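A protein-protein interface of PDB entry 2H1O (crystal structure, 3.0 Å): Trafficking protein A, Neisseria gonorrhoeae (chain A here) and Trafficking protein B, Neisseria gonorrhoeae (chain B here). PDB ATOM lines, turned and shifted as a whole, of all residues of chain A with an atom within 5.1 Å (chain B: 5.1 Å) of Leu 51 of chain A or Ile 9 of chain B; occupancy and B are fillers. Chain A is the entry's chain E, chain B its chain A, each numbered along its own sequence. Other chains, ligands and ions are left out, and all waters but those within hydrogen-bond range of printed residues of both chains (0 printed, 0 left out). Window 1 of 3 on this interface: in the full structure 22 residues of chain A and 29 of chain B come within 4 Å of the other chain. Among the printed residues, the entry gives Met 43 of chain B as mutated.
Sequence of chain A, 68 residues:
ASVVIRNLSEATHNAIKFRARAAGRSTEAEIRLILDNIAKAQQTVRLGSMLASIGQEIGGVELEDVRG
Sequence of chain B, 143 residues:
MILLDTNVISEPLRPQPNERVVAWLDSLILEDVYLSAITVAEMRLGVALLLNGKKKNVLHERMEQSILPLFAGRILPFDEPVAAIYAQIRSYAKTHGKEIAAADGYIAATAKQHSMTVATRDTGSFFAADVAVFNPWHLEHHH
Printed residues of chain B that touch a printed residue of chain A: Leu 4, Ile 9, Pro 12, Leu 13, Leu 25, Ile 67 and Phe 71. Hydrophobic or aromatic side chains of chain B that line the printed part of chain A: Leu 4, Ile 9, Pro 12, Leu 13, Leu 25, Ile 67 and Phe 71. Among the printed residues, 10 pairs touch across the chains.
CD2 of Leu 47 of chain A touches CD1 of Leu 4 of chain B, 3.9 Å away. CD2 of Leu 47 of chain A touches CZ of Phe 71 of chain B (3.6 Å). Gly 48 of chain A touches Leu 25 of chain B. CD1 of Leu 51 of chain A touches CD1 of Ile 9 of chain B (3.4 Å). Pro 12 of chain B touches Leu 51 of chain A (CB to CB, 3.5 Å). Leu 51 of chain A touches Leu 13 of chain B. CG2 of Ile 67 of chain B touches CD2 of Leu 51 of chain A, at 3.6 Å. Ala 52 of chain A touches Pro 12 of chain B (N to CB, 3.7 Å). CG2 of Ile 54 of chain A touches CD2 of Leu 13 of chain B (3.5 Å). Gly 55 of chain A touches Leu 13 of chain B (CA to O, 3.8 Å).
Printed residues of chain B within 4 Å of Leu 51 of chain A: Ile 9 (3.4 Å), Pro 12 (3.5 Å), Leu 13 (3.4 Å) and Ile 67 (3.6 Å). Printed residues of chain A within 4 Å of Leu 25 of chain B: Gly 48 (3.3 Å). Of the printed residues of chain B, Leu 47 of chain A touches Leu 4 (3.9 Å) and Phe 71 (3.6 Å). Printed residues of chain B within 4 Å of Gly 55 of chain A: Leu 13. Of the printed residues of chain A, Phe 71 of chain B touches Leu 47. The nearest printed residue of chain A that does not touch Ile 9 of chain B is Leu 47 of chain A (5.5 Å). The nearest printed residue of chain A that does not touch Pro 12 of chain B is Gly 48 of chain A (4.1 Å).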
ATOM      1  N   ARG A  46     -29.764 -16.944  11.213  1.00  0.00           N
ATOM      2  CA  ARG A  46     -28.339 -16.865  11.473  1.00  0.00           C
ATOM      3  C   ARG A  46     -28.147 -16.167  12.814  1.00  0.00           C
ATOM      4  O   ARG A  46     -28.142 -14.941  12.900  1.00  0.00           O
ATOM      5  CB  ARG A  46     -27.640 -16.102  10.345  1.00  0.00           C
ATOM      6  CG  ARG A  46     -27.739 -16.779   8.968  1.00  0.00           C
ATOM      7  CD  ARG A  46     -26.478 -16.542   8.137  1.00  0.00           C
ATOM      8  NE  ARG A  46     -26.102 -15.129   8.124  1.00  0.00           N
ATOM      9  CZ  ARG A  46     -24.935 -14.665   7.685  1.00  0.00           C
ATOM     10  NH1 ARG A  46     -24.023 -15.515   7.222  1.00  0.00           N
ATOM     11  NH2 ARG A  46     -24.677 -13.355   7.715  1.00  0.00           N
ATOM     12  N   LEU A  47     -27.983 -16.966  13.861  1.00  0.00           N
ATOM     13  CA  LEU A  47     -27.845 -16.444  15.209  1.00  0.00           C
ATOM     14  C   LEU A  47     -26.833 -15.314  15.362  1.00  0.00           C
ATOM     15  O   LEU A  47     -27.138 -14.283  15.960  1.00  0.00           O
ATOM     16  CB  LEU A  47     -27.512 -17.584  16.166  1.00  0.00           C
ATOM     17  CG  LEU A  47     -27.806 -17.234  17.621  1.00  0.00           C
ATOM     18  CD1 LEU A  47     -29.284 -16.867  17.779  1.00  0.00           C
ATOM     19  CD2 LEU A  47     -27.425 -18.404  18.510  1.00  0.00           C
ATOM     20  N   GLY A  48     -25.631 -15.504  14.828  1.00  0.00           N
ATOM     21  CA  GLY A  48     -24.616 -14.470  14.927  1.00  0.00           C
ATOM     22  C   GLY A  48     -25.108 -13.104  14.479  1.00  0.00           C
ATOM     23  O   GLY A  48     -25.294 -12.199  15.288  1.00  0.00           O
ATOM     24  N   SER A  49     -25.327 -12.960  13.179  1.00  0.00           N
ATOM     25  CA  SER A  49     -25.803 -11.712  12.603  1.00  0.00           C
ATOM     26  C   SER A  49     -27.060 -11.203  13.290  1.00  0.00           C
ATOM     27  O   SER A  49     -27.296  -9.997  13.363  1.00  0.00           O
ATOM     28  CB  SER A  49     -26.091 -11.904  11.119  1.00  0.00           C
ATOM     29  OG  SER A  49     -24.934 -12.344  10.435  1.00  0.00           O
ATOM     30  N   MET A  50     -27.868 -12.128  13.790  1.00  0.00           N
ATOM     31  CA  MET A  50     -29.114 -11.785  14.466  1.00  0.00           C
ATOM     32  C   MET A  50     -28.818 -10.970  15.722  1.00  0.00           C
ATOM     33  O   MET A  50     -29.295  -9.845  15.881  1.00  0.00           O
ATOM     34  CB  MET A  50     -29.858 -13.070  14.825  1.00  0.00           C
ATOM     35  CG  MET A  50     -31.354 -13.013  14.607  1.00  0.00           C
ATOM     36  SD  MET A  50     -32.145 -11.831  15.698  1.00  0.00           S
ATOM     37  CE  MET A  50     -31.908 -12.666  17.323  1.00  0.00           C
ATOM     38  N   LEU A  51     -28.012 -11.546  16.607  1.00  0.00           N
ATOM     39  CA  LEU A  51     -27.635 -10.889  17.847  1.00  0.00           C
ATOM     40  C   LEU A  51     -26.862  -9.603  17.563  1.00  0.00           C
ATOM     41  O   LEU A  51     -26.988  -8.610  18.281  1.00  0.00           O
ATOM     42  CB  LEU A  51     -26.792 -11.846  18.699  1.00  0.00           C
ATOM     43  CG  LEU A  51     -27.560 -13.091  19.163  1.00  0.00           C
ATOM     44  CD1 LEU A  51     -26.612 -14.148  19.705  1.00  0.00           C
ATOM     45  CD2 LEU A  51     -28.590 -12.675  20.208  1.00  0.00           C
ATOM     46  N   ALA A  52     -26.062  -9.625  16.505  1.00  0.00           N
ATOM     47  CA  ALA A  52     -25.276  -8.459  16.138  1.00  0.00           C
ATOM     48  C   ALA A  52     -26.192  -7.283  15.897  1.00  0.00           C
ATOM     49  O   ALA A  52     -25.964  -6.195  16.417  1.00  0.00           O
ATOM     50  CB  ALA A  52     -24.468  -8.743  14.898  1.00  0.00           C
ATOM     51  N   SER A  53     -27.230  -7.498  15.102  1.00  0.00           N
ATOM     52  CA  SER A  53     -28.168  -6.431  14.815  1.00  0.00           C
ATOM     53  C   SER A  53     -28.606  -5.829  16.130  1.00  0.00           C
ATOM     54  O   SER A  53     -28.433  -4.636  16.360  1.00  0.00           O
ATOM     55  CB  SER A  53     -29.373  -6.974  14.059  1.00  0.00           C
ATOM     56  OG  SER A  53     -28.970  -7.492  12.805  1.00  0.00           O
ATOM     57  N   ILE A  54     -29.163  -6.671  16.996  1.00  0.00           N
ATOM     58  CA  ILE A  54     -29.621  -6.227  18.307  1.00  0.00           C
ATOM     59  C   ILE A  54     -28.529  -5.377  18.932  1.00  0.00           C
ATOM     60  O   ILE A  54     -28.803  -4.396  19.607  1.00  0.00           O
ATOM     61  CB  ILE A  54     -29.875  -7.402  19.264  1.00  0.00           C
ATOM     62  CG1 ILE A  54     -30.886  -8.381  18.664  1.00  0.00           C
ATOM     63  CG2 ILE A  54     -30.357  -6.864  20.602  1.00  0.00           C
ATOM     64  CD1 ILE A  54     -32.314  -7.909  18.723  1.00  0.00           C
ATOM     65  N   GLY A  55     -27.283  -5.772  18.714  1.00  0.00           N
ATOM     66  CA  GLY A  55     -26.181  -5.016  19.266  1.00  0.00           C
ATOM     67  C   GLY A  55     -26.122  -3.644  18.634  1.00  0.00           C
ATOM     68  O   GLY A  55     -26.096  -2.641  19.339  1.00  0.00           O
ATOM     69  N   LEU B   4     -24.407 -22.959  24.370  1.00  0.00           N
ATOM     70  CA  LEU B   4     -23.779 -21.653  24.432  1.00  0.00           C
ATOM     71  C   LEU B   4     -23.659 -21.148  25.857  1.00  0.00           C
ATOM     72  O   LEU B   4     -24.620 -21.128  26.623  1.00  0.00           O
ATOM     73  CB  LEU B   4     -24.555 -20.632  23.600  1.00  0.00           C
ATOM     74  CG  LEU B   4     -24.606 -20.916  22.106  1.00  0.00           C
ATOM     75  CD1 LEU B   4     -25.063 -19.689  21.380  1.00  0.00           C
ATOM     76  CD2 LEU B   4     -23.239 -21.309  21.619  1.00  0.00           C
ATOM     77  N   ASP B   5     -22.456 -20.739  26.218  1.00  0.00           N
ATOM     78  CA  ASP B   5     -22.240 -20.220  27.540  1.00  0.00           C
ATOM     79  C   ASP B   5     -22.440 -18.712  27.411  1.00  0.00           C
ATOM     80  O   ASP B   5     -22.225 -18.135  26.336  1.00  0.00           O
ATOM     81  CB  ASP B   5     -20.827 -20.564  28.000  1.00  0.00           C
ATOM     82  CG  ASP B   5     -20.669 -20.493  29.505  1.00  0.00           C
ATOM     83  OD1 ASP B   5     -21.679 -20.235  30.200  1.00  0.00           O
ATOM     84  OD2 ASP B   5     -19.531 -20.699  29.992  1.00  0.00           O
ATOM     85  N   THR B   6     -22.864 -18.092  28.509  1.00  0.00           N
ATOM     86  CA  THR B   6     -23.131 -16.660  28.578  1.00  0.00           C
ATOM     87  C   THR B   6     -22.242 -15.761  27.730  1.00  0.00           C
ATOM     88  O   THR B   6     -22.731 -15.044  26.855  1.00  0.00           O
ATOM     89  CB  THR B   6     -23.032 -16.176  30.017  1.00  0.00           C
ATOM     90  OG1 THR B   6     -23.789 -17.052  30.854  1.00  0.00           O
ATOM     91  CG2 THR B   6     -23.586 -14.773  30.145  1.00  0.00           C
ATOM     92  N   ASN B   7     -20.940 -15.796  27.981  1.00  0.00           N
ATOM     93  CA  ASN B   7     -20.013 -14.941  27.252  1.00  0.00           C
ATOM     94  C   ASN B   7     -20.030 -15.020  25.721  1.00  0.00           C
ATOM     95  O   ASN B   7     -19.591 -14.086  25.054  1.00  0.00           O
ATOM     96  CB  ASN B   7     -18.590 -15.143  27.783  1.00  0.00           C
ATOM     97  CG  ASN B   7     -18.046 -16.512  27.485  1.00  0.00           C
ATOM     98  OD1 ASN B   7     -17.504 -16.753  26.408  1.00  0.00           O
ATOM     99  ND2 ASN B   7     -18.197 -17.431  28.437  1.00  0.00           N
ATOM    100  N   VAL B   8     -20.527 -16.101  25.137  1.00  0.00           N
ATOM    101  CA  VAL B   8     -20.553 -16.120  23.682  1.00  0.00           C
ATOM    102  C   VAL B   8     -21.792 -15.380  23.219  1.00  0.00           C
ATOM    103  O   VAL B   8     -21.703 -14.422  22.468  1.00  0.00           O
ATOM    104  CB  VAL B   8     -20.553 -17.541  23.106  1.00  0.00           C
ATOM    105  CG1 VAL B   8     -20.653 -17.471  21.606  1.00  0.00           C
ATOM    106  CG2 VAL B   8     -19.262 -18.259  23.494  1.00  0.00           C
ATOM    107  N   ILE B   9     -22.947 -15.812  23.694  1.00  0.00           N
ATOM    108  CA  ILE B   9     -24.218 -15.183  23.355  1.00  0.00           C
ATOM    109  C   ILE B   9     -24.131 -13.656  23.567  1.00  0.00           C
ATOM    110  O   ILE B   9     -24.896 -12.896  22.985  1.00  0.00           O
ATOM    111  CB  ILE B   9     -25.345 -15.782  24.243  1.00  0.00           C
ATOM    112  CG1 ILE B   9     -26.615 -16.021  23.420  1.00  0.00           C
ATOM    113  CG2 ILE B   9     -25.618 -14.864  25.432  1.00  0.00           C
ATOM    114  CD1 ILE B   9     -27.305 -14.772  22.953  1.00  0.00           C
ATOM    115  N   SER B  10     -23.194 -13.215  24.400  1.00  0.00           N
ATOM    116  CA  SER B  10     -23.018 -11.792  24.681  1.00  0.00           C
ATOM    117  C   SER B  10     -22.150 -11.089  23.653  1.00  0.00           C
ATOM    118  O   SER B  10     -22.392  -9.929  23.314  1.00  0.00           O
ATOM    119  CB  SER B  10     -22.348 -11.582  26.037  1.00  0.00           C
ATOM    120  OG  SER B  10     -23.142 -12.040  27.105  1.00  0.00           O
ATOM    121  N   GLU B  11     -21.130 -11.788  23.165  1.00  0.00           N
ATOM    122  CA  GLU B  11     -20.204 -11.188  22.217  1.00  0.00           C
ATOM    123  C   GLU B  11     -20.783 -10.310  21.113  1.00  0.00           C
ATOM    124  O   GLU B  11     -20.329  -9.185  20.926  1.00  0.00           O
ATOM    125  CB  GLU B  11     -19.299 -12.239  21.583  1.00  0.00           C
ATOM    126  CG  GLU B  11     -18.128 -11.596  20.858  1.00  0.00           C
ATOM    127  CD  GLU B  11     -17.247 -10.756  21.790  1.00  0.00           C
ATOM    128  OE1 GLU B  11     -16.428  -9.949  21.296  1.00  0.00           O
ATOM    129  OE2 GLU B  11     -17.365 -10.915  23.024  1.00  0.00           O
ATOM    130  N   PRO B  12     -21.794 -10.789  20.376  1.00  0.00           N
ATOM    131  CA  PRO B  12     -22.358  -9.962  19.302  1.00  0.00           C
ATOM    132  C   PRO B  12     -23.006  -8.663  19.783  1.00  0.00           C
ATOM    133  O   PRO B  12     -22.951  -7.638  19.108  1.00  0.00           O
ATOM    134  CB  PRO B  12     -23.385 -10.889  18.649  1.00  0.00           C
ATOM    135  CG  PRO B  12     -22.935 -12.255  19.044  1.00  0.00           C
ATOM    136  CD  PRO B  12     -22.503 -12.071  20.463  1.00  0.00           C
ATOM    137  N   LEU B  13     -23.626  -8.724  20.955  1.00  0.00           N
ATOM    138  CA  LEU B  13     -24.322  -7.585  21.532  1.00  0.00           C
ATOM    139  C   LEU B  13     -23.391  -6.487  21.967  1.00  0.00           C
ATOM    140  O   LEU B  13     -23.831  -5.372  22.230  1.00  0.00           O
ATOM    141  CB  LEU B  13     -25.139  -8.034  22.736  1.00  0.00           C
ATOM    142  CG  LEU B  13     -26.311  -8.966  22.447  1.00  0.00           C
ATOM    143  CD1 LEU B  13     -26.887  -9.456  23.753  1.00  0.00           C
ATOM    144  CD2 LEU B  13     -27.360  -8.238  21.624  1.00  0.00           C
ATOM    145  N   LEU B  25     -21.135 -18.184  14.829  1.00  0.00           N
ATOM    146  CA  LEU B  25     -22.528 -18.316  15.239  1.00  0.00           C
ATOM    147  C   LEU B  25     -23.421 -18.441  14.008  1.00  0.00           C
ATOM    148  O   LEU B  25     -24.428 -19.150  14.025  1.00  0.00           O
ATOM    149  CB  LEU B  25     -22.968 -17.116  16.084  1.00  0.00           C
ATOM    150  CG  LEU B  25     -22.554 -17.079  17.564  1.00  0.00           C
ATOM    151  CD1 LEU B  25     -22.795 -15.695  18.127  1.00  0.00           C
ATOM    152  CD2 LEU B  25     -23.331 -18.104  18.356  1.00  0.00           C
ATOM    153  N   LEU B  35     -29.284 -23.432  25.449  1.00  0.00           N
ATOM    154  CA  LEU B  35     -28.875 -22.531  26.528  1.00  0.00           C
ATOM    155  C   LEU B  35     -29.210 -23.183  27.861  1.00  0.00           C
ATOM    156  O   LEU B  35     -30.191 -23.924  27.954  1.00  0.00           O
ATOM    157  CB  LEU B  35     -29.638 -21.209  26.458  1.00  0.00           C
ATOM    158  CG  LEU B  35     -29.345 -20.311  25.277  1.00  0.00           C
ATOM    159  CD1 LEU B  35     -30.177 -19.071  25.365  1.00  0.00           C
ATOM    160  CD2 LEU B  35     -27.882 -19.978  25.277  1.00  0.00           C
ATOM    161  N   MET B  43     -28.044 -13.819  31.754  1.00  0.00           N
ATOM    162  CA  MET B  43     -28.397 -12.827  30.750  1.00  0.00           C
ATOM    163  C   MET B  43     -29.471 -11.915  31.312  1.00  0.00           C
ATOM    164  O   MET B  43     -29.327 -10.692  31.319  1.00  0.00           O
ATOM    165  CB  MET B  43     -28.951 -13.501  29.504  1.00  0.00           C
ATOM    166  CG  MET B  43     -27.926 -14.027  28.532  1.00  0.00           C
ATOM    167  SD  MET B  43     -28.761 -15.088  27.297  1.00  0.00           S
ATOM    168  CE  MET B  43     -29.374 -13.867  26.096  1.00  0.00           C
ATOM    169  N   ILE B  67     -34.413 -12.697  20.954  1.00  0.00           N
ATOM    170  CA  ILE B  67     -33.410 -13.682  21.310  1.00  0.00           C
ATOM    171  C   ILE B  67     -34.036 -14.943  21.901  1.00  0.00           C
ATOM    172  O   ILE B  67     -34.408 -15.851  21.162  1.00  0.00           O
ATOM    173  CB  ILE B  67     -32.419 -13.111  22.318  1.00  0.00           C
ATOM    174  CG1 ILE B  67     -32.040 -11.687  21.914  1.00  0.00           C
ATOM    175  CG2 ILE B  67     -31.176 -13.979  22.351  1.00  0.00           C
ATOM    176  CD1 ILE B  67     -31.294 -10.928  22.984  1.00  0.00           C
ATOM    177  N   PHE B  71     -34.876 -20.026  21.410  1.00  0.00           N
ATOM    178  CA  PHE B  71     -34.328 -21.198  22.051  1.00  0.00           C
ATOM    179  C   PHE B  71     -35.425 -21.921  22.812  1.00  0.00           C
ATOM    180  O   PHE B  71     -35.143 -22.751  23.678  1.00  0.00           O
ATOM    181  CB  PHE B  71     -33.222 -20.796  23.011  1.00  0.00           C
ATOM    182  CG  PHE B  71     -32.041 -20.154  22.345  1.00  0.00           C
ATOM    183  CD1 PHE B  71     -32.090 -18.829  21.932  1.00  0.00           C
ATOM    184  CD2 PHE B  71     -30.852 -20.869  22.169  1.00  0.00           C
ATOM    185  CE1 PHE B  71     -30.971 -18.221  21.362  1.00  0.00           C
ATOM    186  CE2 PHE B  71     -29.730 -20.273  21.600  1.00  0.00           C
ATOM    187  CZ  PHE B  71     -29.788 -18.947  21.198  1.00  0.00           C
